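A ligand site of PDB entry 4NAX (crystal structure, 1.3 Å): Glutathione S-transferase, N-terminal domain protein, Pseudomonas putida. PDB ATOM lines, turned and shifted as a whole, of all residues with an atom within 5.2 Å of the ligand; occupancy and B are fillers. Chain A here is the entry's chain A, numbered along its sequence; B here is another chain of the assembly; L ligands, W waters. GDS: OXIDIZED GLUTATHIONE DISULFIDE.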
ATOM      1  N   THR A  28     -12.056  21.095  22.729  1.00  0.00           N
ATOM      2  CA  THR A  28     -12.366  21.664  24.014  1.00  0.00           C
ATOM      3  C   THR A  28     -11.649  20.789  25.041  1.00  0.00           C
ATOM      4  O   THR A  28     -11.218  19.697  24.713  1.00  0.00           O
ATOM      5  CB  THR A  28     -13.848  21.563  24.313  1.00  0.00           C
ATOM      6  OG1 THR A  28     -14.206  20.167  24.307  1.00  0.00           O
ATOM      7  CG2 THR A  28     -14.720  22.286  23.306  1.00  0.00           C
ATOM      8  N   PRO A  29     -11.572  21.213  26.308  1.00  0.00           N
ATOM      9  CA  PRO A  29     -10.816  20.381  27.226  1.00  0.00           C
ATOM     10  C   PRO A  29     -11.384  18.983  27.395  1.00  0.00           C
ATOM     11  O   PRO A  29     -10.621  18.061  27.641  1.00  0.00           O
ATOM     12  CB  PRO A  29     -10.866  21.170  28.553  1.00  0.00           C
ATOM     13  CG  PRO A  29     -11.991  22.163  28.361  1.00  0.00           C
ATOM     14  CD  PRO A  29     -11.897  22.519  26.899  1.00  0.00           C
ATOM     15  N   ASN A  30     -12.708  18.829  27.306  1.00  0.00           N
ATOM     16  CA  ASN A  30     -13.287  17.501  27.357  1.00  0.00           C
ATOM     17  C   ASN A  30     -13.189  16.710  26.067  1.00  0.00           C
ATOM     18  O   ASN A  30     -12.931  15.522  26.079  1.00  0.00           O
ATOM     19  CB  ASN A  30     -14.716  17.576  27.859  1.00  0.00           C
ATOM     20  CG  ASN A  30     -14.757  18.091  29.277  1.00  0.00           C
ATOM     21  OD1 ASN A  30     -13.993  17.642  30.137  1.00  0.00           O
ATOM     22  ND2 ASN A  30     -15.630  19.041  29.540  1.00  0.00           N
ATOM     23  N   GLY A  31     -13.419  17.379  24.928  1.00  0.00           N
ATOM     24  CA  GLY A  31     -13.298  16.709  23.650  1.00  0.00           C
ATOM     25  C   GLY A  31     -11.913  16.172  23.398  1.00  0.00           C
ATOM     26  O   GLY A  31     -11.731  15.053  22.922  1.00  0.00           O
ATOM     27  N   LYS A  33      -9.675  15.183  25.437  1.00  0.00           N
ATOM     28  CA  LYS A  33      -9.313  13.987  26.200  1.00  0.00           C
ATOM     29  C   LYS A  33      -9.442  12.772  25.264  1.00  0.00           C
ATOM     30  O   LYS A  33      -8.604  11.880  25.284  1.00  0.00           O
ATOM     31  CB  LYS A  33     -10.266  13.775  27.372  1.00  0.00           C
ATOM     32  CG  LYS A  33     -10.236  14.818  28.469  1.00  0.00           C
ATOM     33  CD  LYS A  33     -11.360  14.533  29.448  1.00  0.00           C
ATOM     34  CE  LYS A  33     -11.562  15.590  30.518  1.00  0.00           C
ATOM     35  NZ  LYS A  33     -12.782  15.266  31.341  1.00  0.00           N
ATOM     36  N   PHE A  52     -21.018  24.136  18.114  1.00  0.00           N
ATOM     37  CA  PHE A  52     -21.906  24.832  19.060  1.00  0.00           C
ATOM     38  C   PHE A  52     -22.544  26.086  18.422  1.00  0.00           C
ATOM     39  O   PHE A  52     -23.660  26.465  18.772  1.00  0.00           O
ATOM     40  CB  PHE A  52     -21.152  25.231  20.327  1.00  0.00           C
ATOM     41  CG  PHE A  52     -20.654  24.057  21.152  1.00  0.00           C
ATOM     42  CD1 PHE A  52     -21.059  22.752  20.907  1.00  0.00           C
ATOM     43  CD2 PHE A  52     -19.754  24.289  22.190  1.00  0.00           C
ATOM     44  CE1 PHE A  52     -20.591  21.706  21.683  1.00  0.00           C
ATOM     45  CE2 PHE A  52     -19.290  23.256  22.968  1.00  0.00           C
ATOM     46  CZ  PHE A  52     -19.705  21.965  22.719  1.00  0.00           C
ATOM     47  N   GLN A  57     -25.100  20.398  19.032  1.00  0.00           N
ATOM     48  CA  GLN A  57     -25.172  19.545  20.209  1.00  0.00           C
ATOM     49  C   GLN A  57     -26.590  19.512  20.790  1.00  0.00           C
ATOM     50  O   GLN A  57     -26.905  18.690  21.629  1.00  0.00           O
ATOM     51  CB  GLN A  57     -24.155  19.968  21.290  1.00  0.00           C
ATOM     52  CG  GLN A  57     -24.535  21.158  22.162  1.00  0.00           C
ATOM     53  CD  GLN A  57     -24.476  22.533  21.512  1.00  0.00           C
ATOM     54  OE1 GLN A  57     -24.365  22.686  20.295  1.00  0.00           O
ATOM     55  NE2 GLN A  57     -24.553  23.544  22.352  1.00  0.00           N
ATOM     56  N   LEU A  58     -27.431  20.436  20.341  1.00  0.00           N
ATOM     57  CA  LEU A  58     -28.840  20.453  20.743  1.00  0.00           C
ATOM     58  C   LEU A  58     -29.770  19.782  19.717  1.00  0.00           C
ATOM     59  O   LEU A  58     -30.992  19.724  19.929  1.00  0.00           O
ATOM     60  CB  LEU A  58     -29.313  21.875  20.982  1.00  0.00           C
ATOM     61  CG  LEU A  58     -28.533  22.649  22.049  1.00  0.00           C
ATOM     62  CD1 LEU A  58     -28.984  24.089  22.182  1.00  0.00           C
ATOM     63  CD2 LEU A  58     -28.615  21.975  23.407  1.00  0.00           C
ATOM     64  N   ASN A  69     -26.710  16.170  25.818  1.00  0.00           N
ATOM     65  CA  ASN A  69     -26.474  17.251  24.874  1.00  0.00           C
ATOM     66  C   ASN A  69     -25.062  17.824  24.896  1.00  0.00           C
ATOM     67  O   ASN A  69     -24.863  18.983  24.567  1.00  0.00           O
ATOM     68  CB  ASN A  69     -27.604  18.308  24.809  1.00  0.00           C
ATOM     69  CG  ASN A  69     -27.736  19.225  26.014  1.00  0.00           C
ATOM     70  OD1 ASN A  69     -28.727  19.127  26.756  1.00  0.00           O
ATOM     71  ND2 ASN A  69     -26.844  20.183  26.140  1.00  0.00           N
ATOM     72  N   LYS A  70     -24.089  16.980  25.240  1.00  0.00           N
ATOM     73  CA  LYS A  70     -22.707  17.435  25.339  1.00  0.00           C
ATOM     74  C   LYS A  70     -21.748  16.586  24.556  1.00  0.00           C
ATOM     75  O   LYS A  70     -21.994  15.404  24.303  1.00  0.00           O
ATOM     76  CB  LYS A  70     -22.306  17.577  26.810  1.00  0.00           C
ATOM     77  CG  LYS A  70     -23.125  18.712  27.470  1.00  0.00           C
ATOM     78  CD  LYS A  70     -22.722  19.196  28.808  1.00  0.00           C
ATOM     79  CE  LYS A  70     -23.697  20.269  29.231  1.00  0.00           C
ATOM     80  NZ  LYS A  70     -23.324  20.876  30.508  1.00  0.00           N
ATOM     81  N   ILE A  71     -20.661  17.211  24.136  1.00  0.00           N
ATOM     82  CA  ILE A  71     -19.541  16.482  23.566  1.00  0.00           C
ATOM     83  C   ILE A  71     -18.522  16.221  24.670  1.00  0.00           C
ATOM     84  O   ILE A  71     -18.467  16.946  25.676  1.00  0.00           O
ATOM     85  CB  ILE A  71     -18.907  17.249  22.365  1.00  0.00           C
ATOM     86  CG1 ILE A  71     -18.253  18.580  22.757  1.00  0.00           C
ATOM     87  CG2 ILE A  71     -19.916  17.446  21.255  1.00  0.00           C
ATOM     88  CD1 ILE A  71     -16.812  18.486  23.234  1.00  0.00           C
ATOM     89  N   PRO A  72     -17.649  15.221  24.479  1.00  0.00           N
ATOM     90  CA  PRO A  72     -17.593  14.277  23.364  1.00  0.00           C
ATOM     91  C   PRO A  72     -18.577  13.106  23.505  1.00  0.00           C
ATOM     92  O   PRO A  72     -19.046  12.784  24.604  1.00  0.00           O
ATOM     93  CB  PRO A  72     -16.165  13.755  23.445  1.00  0.00           C
ATOM     94  CG  PRO A  72     -15.874  13.744  24.919  1.00  0.00           C
ATOM     95  CD  PRO A  72     -16.562  14.995  25.446  1.00  0.00           C
ATOM     96  N   GLU A  89     -19.865  10.964  27.883  1.00  0.00           N
ATOM     97  CA  GLU A  89     -19.040  11.279  29.059  1.00  0.00           C
ATOM     98  C   GLU A  89     -17.575  10.960  28.772  1.00  0.00           C
ATOM     99  O   GLU A  89     -17.185   9.798  28.655  1.00  0.00           O
ATOM    100  CB  GLU A  89     -19.478  10.589  30.345  1.00  0.00           C
ATOM    101  CG  GLU A  89     -20.809  11.091  30.867  1.00  0.00           C
ATOM    102  CD  GLU A  89     -20.763  12.530  31.354  1.00  0.00           C
ATOM    103  OE1 GLU A  89     -19.716  12.946  31.905  1.00  0.00           O
ATOM    104  OE2 GLU A  89     -21.798  13.224  31.176  1.00  0.00           O
ATOM    105  N   SER A  90     -16.765  12.014  28.667  1.00  0.00           N
ATOM    106  CA  SER A  90     -15.355  11.846  28.369  1.00  0.00           C
ATOM    107  C   SER A  90     -14.679  10.801  29.251  1.00  0.00           C
ATOM    108  O   SER A  90     -13.929   9.960  28.753  1.00  0.00           O
ATOM    109  CB  SER A  90     -14.636  13.182  28.462  1.00  0.00           C
ATOM    110  OG  SER A  90     -14.587  13.671  29.780  1.00  0.00           O
ATOM    111  N   GLY A  91     -14.925  10.858  30.559  1.00  0.00           N
ATOM    112  CA  GLY A  91     -14.269   9.922  31.467  1.00  0.00           C
ATOM    113  C   GLY A  91     -14.698   8.480  31.253  1.00  0.00           C
ATOM    114  O   GLY A  91     -13.893   7.561  31.459  1.00  0.00           O
ATOM    115  N   MET A 123     -13.031  14.329  37.042  1.00  0.00           N
ATOM    116  CA  MET A 123     -14.390  14.463  36.539  1.00  0.00           C
ATOM    117  C   MET A 123     -15.295  15.244  37.484  1.00  0.00           C
ATOM    118  O   MET A 123     -16.191  15.949  37.030  1.00  0.00           O
ATOM    119  CB  MET A 123     -14.977  13.099  36.210  1.00  0.00           C
ATOM    120  CG  MET A 123     -14.379  12.457  34.942  1.00  0.00           C
ATOM    121  SD  MET A 123     -14.822  13.229  33.391  1.00  0.00           S
ATOM    122  CE  MET A 123     -16.535  12.766  33.292  1.00  0.00           C
ATOM    123  N   GLY A 127     -12.587  19.366  36.216  1.00  0.00           N
ATOM    124  CA  GLY A 127     -13.414  19.874  35.108  1.00  0.00           C
ATOM    125  C   GLY A 127     -14.480  20.864  35.583  1.00  0.00           C
ATOM    126  O   GLY A 127     -14.580  21.972  35.088  1.00  0.00           O
ATOM    127  N   PRO A 128     -15.306  20.438  36.560  1.00  0.00           N
ATOM    128  CA  PRO A 128     -16.417  21.307  36.947  1.00  0.00           C
ATOM    129  C   PRO A 128     -15.926  22.629  37.539  1.00  0.00           C
ATOM    130  O   PRO A 128     -16.488  23.671  37.231  1.00  0.00           O
ATOM    131  CB  PRO A 128     -17.165  20.446  37.984  1.00  0.00           C
ATOM    132  CG  PRO A 128     -16.961  19.041  37.490  1.00  0.00           C
ATOM    133  CD  PRO A 128     -15.504  19.045  37.040  1.00  0.00           C
ATOM    134  N   GLY A 131     -13.992  24.875  35.009  1.00  0.00           N
ATOM    135  CA  GLY A 131     -14.982  25.423  34.112  1.00  0.00           C
ATOM    136  C   GLY A 131     -15.704  26.627  34.688  1.00  0.00           C
ATOM    137  O   GLY A 131     -16.053  27.547  33.957  1.00  0.00           O
ATOM    138  N   GLN A 132     -15.933  26.648  36.009  1.00  0.00           N
ATOM    139  CA  GLN A 132     -16.563  27.806  36.638  1.00  0.00           C
ATOM    140  C   GLN A 132     -15.629  29.006  36.669  1.00  0.00           C
ATOM    141  O   GLN A 132     -16.091  30.139  36.565  1.00  0.00           O
ATOM    142  CB  GLN A 132     -17.096  27.501  38.036  1.00  0.00           C
ATOM    143  CG  GLN A 132     -18.041  26.308  38.154  1.00  0.00           C
ATOM    144  CD  GLN A 132     -18.964  26.176  36.979  1.00  0.00           C
ATOM    145  OE1 GLN A 132     -19.781  27.061  36.704  1.00  0.00           O
ATOM    146  NE2 GLN A 132     -18.844  25.078  36.271  1.00  0.00           N
ATOM    147  N   PHE A 135     -16.170  30.570  33.440  1.00  0.00           N
ATOM    148  CA  PHE A 135     -17.381  31.382  33.397  1.00  0.00           C
ATOM    149  C   PHE A 135     -17.185  32.753  34.049  1.00  0.00           C
ATOM    150  O   PHE A 135     -17.607  33.771  33.495  1.00  0.00           O
ATOM    151  CB  PHE A 135     -18.572  30.687  34.060  1.00  0.00           C
ATOM    152  CG  PHE A 135     -19.833  31.480  33.928  1.00  0.00           C
ATOM    153  CD1 PHE A 135     -20.437  31.625  32.679  1.00  0.00           C
ATOM    154  CD2 PHE A 135     -20.366  32.181  35.003  1.00  0.00           C
ATOM    155  CE1 PHE A 135     -21.553  32.423  32.517  1.00  0.00           C
ATOM    156  CE2 PHE A 135     -21.478  32.970  34.852  1.00  0.00           C
ATOM    157  CZ  PHE A 135     -22.078  33.085  33.615  1.00  0.00           C
ATOM    158  N   TRP A 188      -7.293  20.132  30.919  1.00  0.00           N
ATOM    159  CA  TRP A 188      -7.991  21.111  31.749  1.00  0.00           C
ATOM    160  C   TRP A 188      -7.045  22.122  32.392  1.00  0.00           C
ATOM    161  O   TRP A 188      -7.368  23.302  32.500  1.00  0.00           O
ATOM    162  CB  TRP A 188      -8.876  20.424  32.785  1.00  0.00           C
ATOM    163  CG  TRP A 188     -10.288  20.286  32.321  1.00  0.00           C
ATOM    164  CD1 TRP A 188     -10.949  19.165  31.938  1.00  0.00           C
ATOM    165  CD2 TRP A 188     -11.202  21.368  32.170  1.00  0.00           C
ATOM    166  NE1 TRP A 188     -12.256  19.477  31.584  1.00  0.00           N
ATOM    167  CE2 TRP A 188     -12.423  20.835  31.738  1.00  0.00           C
ATOM    168  CE3 TRP A 188     -11.103  22.753  32.372  1.00  0.00           C
ATOM    169  CZ2 TRP A 188     -13.537  21.621  31.520  1.00  0.00           C
ATOM    170  CZ3 TRP A 188     -12.202  23.533  32.125  1.00  0.00           C
ATOM    171  CH2 TRP A 188     -13.422  22.966  31.722  1.00  0.00           C
ATOM    172  N   TYR A 196      -8.542  30.383  29.308  1.00  0.00           N
ATOM    173  CA  TYR A 196      -9.281  31.197  30.256  1.00  0.00           C
ATOM    174  C   TYR A 196      -8.490  32.366  30.790  1.00  0.00           C
ATOM    175  O   TYR A 196      -9.040  33.181  31.541  1.00  0.00           O
ATOM    176  CB  TYR A 196      -9.735  30.386  31.453  1.00  0.00           C
ATOM    177  CG  TYR A 196     -10.746  29.321  31.183  1.00  0.00           C
ATOM    178  CD1 TYR A 196     -11.509  29.294  30.014  1.00  0.00           C
ATOM    179  CD2 TYR A 196     -10.998  28.363  32.163  1.00  0.00           C
ATOM    180  CE1 TYR A 196     -12.468  28.318  29.814  1.00  0.00           C
ATOM    181  CE2 TYR A 196     -11.950  27.388  31.970  1.00  0.00           C
ATOM    182  CZ  TYR A 196     -12.683  27.366  30.814  1.00  0.00           C
ATOM    183  OH  TYR A 196     -13.600  26.365  30.644  1.00  0.00           O
ATOM    184  N   MET B 120     -20.462   8.691  35.459  1.00  0.00           N
ATOM    185  CA  MET B 120     -19.718   9.900  35.145  1.00  0.00           C
ATOM    186  C   MET B 120     -20.613  11.117  35.009  1.00  0.00           C
ATOM    187  O   MET B 120     -20.237  12.215  35.419  1.00  0.00           O
ATOM    188  CB  MET B 120     -18.896   9.726  33.884  1.00  0.00           C
ATOM    189  CG  MET B 120     -17.728   8.795  34.074  1.00  0.00           C
ATOM    190  SD  MET B 120     -16.636   9.384  35.406  1.00  0.00           S
ATOM    191  CE  MET B 120     -15.180   8.400  35.180  1.00  0.00           C
ATOM    192  N   GLY B 124     -19.739  14.307  37.313  1.00  0.00           N
ATOM    193  CA  GLY B 124     -19.421  15.619  36.708  1.00  0.00           C
ATOM    194  C   GLY B 124     -20.559  16.621  36.695  1.00  0.00           C
ATOM    195  O   GLY B 124     -20.353  17.823  36.707  1.00  0.00           O
ATOM    196  N   ARG B 152     -27.889  30.292  37.562  1.00  0.00           N
ATOM    197  CA  ARG B 152     -27.054  29.474  36.688  1.00  0.00           C
ATOM    198  C   ARG B 152     -27.099  28.018  37.149  1.00  0.00           C
ATOM    199  O   ARG B 152     -27.327  27.092  36.363  1.00  0.00           O
ATOM    200  CB  ARG B 152     -25.623  30.005  36.679  1.00  0.00           C
ATOM    201  CG  ARG B 152     -24.585  29.114  36.031  1.00  0.00           C
ATOM    202  CD  ARG B 152     -23.215  29.789  36.045  1.00  0.00           C
ATOM    203  NE  ARG B 152     -22.154  28.919  35.554  1.00  0.00           N
ATOM    204  CZ  ARG B 152     -21.922  28.640  34.272  1.00  0.00           C
ATOM    205  NH1 ARG B 152     -22.668  29.160  33.294  1.00  0.00           N
ATOM    206  NH2 ARG B 152     -20.934  27.806  33.975  1.00  0.00           N
HETATM  207  N1  GDS L   1     -23.215  25.235  29.335  1.00  0.00           N
HETATM  208  CA1 GDS L   1     -21.821  25.547  29.625  1.00  0.00           C
HETATM  209  C1  GDS L   1     -21.711  26.709  30.582  1.00  0.00           C
HETATM  210  OE1 GDS L   1     -20.656  26.835  31.238  1.00  0.00           O
HETATM  211  OE2 GDS L   1     -22.650  27.530  30.692  1.00  0.00           O
HETATM  212  CB1 GDS L   1     -21.088  25.871  28.311  1.00  0.00           C
HETATM  213  CG1 GDS L   1     -19.559  25.808  28.408  1.00  0.00           C
HETATM  214  CD1 GDS L   1     -19.073  24.401  28.671  1.00  0.00           C
HETATM  215  O1  GDS L   1     -19.734  23.447  28.307  1.00  0.00           O
HETATM  216  N2  GDS L   1     -17.922  24.308  29.318  1.00  0.00           N
HETATM  217  CA2 GDS L   1     -17.272  23.042  29.596  1.00  0.00           C
HETATM  218  C2  GDS L   1     -17.172  22.782  31.074  1.00  0.00           C
HETATM  219  O2  GDS L   1     -16.931  23.699  31.848  1.00  0.00           O
HETATM  220  CB2 GDS L   1     -15.869  23.047  28.988  1.00  0.00           C
HETATM  221  SG2 GDS L   1     -15.802  23.042  27.196  1.00  0.00           S
HETATM  222  N3  GDS L   1     -17.319  21.528  31.468  1.00  0.00           N
HETATM  223  CA3 GDS L   1     -17.261  21.140  32.869  1.00  0.00           C
HETATM  224  C3  GDS L   1     -16.708  19.745  33.109  1.00  0.00           C
HETATM  225  OE3 GDS L   1     -17.060  19.198  34.177  1.00  0.00           O
HETATM  226  OE4 GDS L   1     -15.917  19.292  32.284  1.00  0.00           O
HETATM  227  N4  GDS L   1     -21.098  21.892  26.107  1.00  0.00           N
HETATM  228  CA4 GDS L   1     -22.261  22.128  25.269  1.00  0.00           C
HETATM  229  C4  GDS L   1     -23.397  22.803  25.998  1.00  0.00           C
HETATM  230  OE5 GDS L   1     -24.442  23.085  25.350  1.00  0.00           O
HETATM  231  OE6 GDS L   1     -23.225  23.091  27.208  1.00  0.00           O
HETATM  232  C5  GDS L   1     -20.350  20.811  25.945  1.00  0.00           C
HETATM  233  O5  GDS L   1     -20.634  19.954  25.112  1.00  0.00           O
HETATM  234  CA5 GDS L   1     -19.115  20.693  26.803  1.00  0.00           C
HETATM  235  N5  GDS L   1     -18.964  19.320  27.278  1.00  0.00           N
HETATM  236  CB5 GDS L   1     -17.906  21.093  25.958  1.00  0.00           C
HETATM  237  SG5 GDS L   1     -16.322  20.935  26.773  1.00  0.00           S
HETATM  238  CA6 GDS L   1     -18.817  15.754  30.653  1.00  0.00           C
HETATM  239  C6  GDS L   1     -17.687  15.012  30.004  1.00  0.00           C
HETATM  240  OE7 GDS L   1     -17.840  14.587  28.839  1.00  0.00           O
HETATM  241  OE8 GDS L   1     -16.644  14.848  30.689  1.00  0.00           O
HETATM  242  N6  GDS L   1     -18.811  15.497  32.111  1.00  0.00           N
HETATM  243  CB6 GDS L   1     -18.701  17.246  30.373  1.00  0.00           C
HETATM  244  CG6 GDS L   1     -18.842  17.558  28.876  1.00  0.00           C
HETATM  245  CD6 GDS L   1     -18.910  19.030  28.580  1.00  0.00           C
HETATM  246  O6  GDS L   1     -18.874  19.879  29.486  1.00  0.00           O
HETATM  247  O   HOH W   1     -19.517  19.622  34.945  1.00  0.00           O
HETATM  248  O   HOH W   2     -26.398  22.553  27.860  1.00  0.00           O
HETATM  249  O   HOH W   3     -18.961  28.988  30.840  1.00  0.00           O
HETATM  250  O   HOH W   4     -19.934  13.887  27.131  1.00  0.00           O
HETATM  251  O   HOH W   5     -16.809  16.435  34.299  1.00  0.00           O
HETATM  252  O   HOH W   6     -14.339  17.048  33.014  1.00  0.00           O
HETATM  253  O   HOH W   7     -23.156  23.667  32.097  1.00  0.00           O
HETATM  254  O   HOH W   8     -20.850  21.662  30.506  1.00  0.00           O
HETATM  255  O   HOH W   9     -15.786  26.544  28.697  1.00  0.00           O
HETATM  256  O   HOH W  10     -24.498  26.116  33.078  1.00  0.00           O
HETATM  257  O   HOH W  11     -18.935  25.359  32.734  1.00  0.00           O
HETATM  258  O   HOH W  12     -25.821  25.264  25.936  1.00  0.00           O
HETATM  259  O   HOH W  13     -25.164  22.999  30.290  1.00  0.00           O
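The side-chain hydroxyl (OG1) of Thr 28 lies close to a sulfur (SG5) of the ligand (3.3 Å). O5 of the ligand is in hydrogen-bond range of N of Ile 71, 2.9 Å away. OE1 of the ligand is in salt-bridge range of NH2 of Arg 152 of chain B (2.9 Å). The side-chain amide nitrogen (NE2) of Gln 57 sits at hydrogen-bond distance from an oxygen (OE5) of the ligand, at 3.0 Å. An oxygen (OE7) of the ligand is in hydrogen-bond range of the backbone NH (N) of Ser 90. An oxygen (OE4) of the ligand sits at hydrogen-bond distance from the side-chain amide nitrogen (ND2) of Asn 30 (2.8 Å). The side-chain amino group (NZ) of Lys 33 lies within salt-bridge range of an oxygen (OE8) of the ligand (3.9 Å). The side-chain carboxylate of Glu 89 lies within salt-bridge range of a nitrogen (N6) of the ligand (2.7 Å). The side-chain hydroxyl (OG) of Ser 90 sits at hydrogen-bond distance from an oxygen (OE8) of the ligand (2.5 Å). The side-chain amino group (NZ) of Lys 70 is in salt-bridge range of an oxygen (OE6) of the ligand (3.98 Å). A nitrogen (N5) of the ligand sits at hydrogen-bond distance from the backbone carbonyl oxygen (O) of Ile 71 (2.9 Å).
The side-chain sulfur (SD) of Met 123 sits close to an oxygen (OE8) of the ligand, at 3.6 Å. N of Pro 128 lies close to OE3 of the ligand, 3.2 Å away. Residues that only touch the ligand: Pro 29 (3.95 Å), Phe 52 (3.3 Å), Asn 69 (3.8 Å), Pro 72 (3.6 Å), Gly 127 (3.4 Å), Gly 131 (3.4 Å) and Trp 188 (3.4 Å). Hydrophobic or aromatic side chains within 4 Å of the ligand: Pro 29, Phe 52, Ile 71, Pro 72, Met 123, Pro 128 and Trp 188. Within 4 Å of the ligand: Thr 28, Pro 29, Asn 30, Lys 33, Phe 52, Gln 57, Asn 69, Lys 70, Ile 71, Pro 72, Glu 89, Ser 90, Met 123, Gly 127, Pro 128, Gly 131, Trp 188 and Arg 152 of chain B. The nearest printed residue that does not touch the ligand is Gly 91 (4.3 Å).
Water W1 lies within hydrogen-bond range of OE3 of the ligand and O of Gly 124 of chain B. Water W4 lies within hydrogen-bond range of OE7 of the ligand, O of Pro 72 and N of Glu 89. Water W6 lies within hydrogen-bond range of an oxygen (OE4) of the ligand, the side-chain amino group of Lys 33 and the side-chain amide oxygen of Asn 30. Water W8 lies within hydrogen-bond range of NZ of Lys 70 (2.6 Å) and O6 of the ligand (2.9 Å). Water W13 lies within hydrogen-bond range of the side-chain amino group of Lys 70 and a nitrogen (N1) of the ligand. Water W9 bridges the side-chain hydroxyl (OH) of Tyr 196 (2.9 Å) and a nitrogen (N2) of the ligand (3.2 Å).
The backbone NH (N) of Gly 91 is in hydrogen-bond range of the side-chain sulfur (SD) of Met 123, 3.7 Å away. The side-chain hydroxyl (OG) of Ser 90 sits at hydrogen-bond distance from the side-chain amino group (NZ) of Lys 33 (2.9 Å). SD of Met 123 lies within hydrogen-bond range of NZ of Lys 33 (3.5 Å). The side-chain amide oxygen of Asn 30 lies within hydrogen-bond range of the indole nitrogen of Trp 188, at 2.9 Å. OG of Ser 90 lies within hydrogen-bond range of SD of Met 123 (3.6 Å). O of Pro 128 sits at hydrogen-bond distance from NE2 of Gln 132, 2.9 Å away. OG1 of Thr 28 lies within hydrogen-bond range of N of Gly 31 (3.0 Å). OD1 of Asn 30 is in hydrogen-bond range of NZ of Lys 33, 2.9 Å away.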
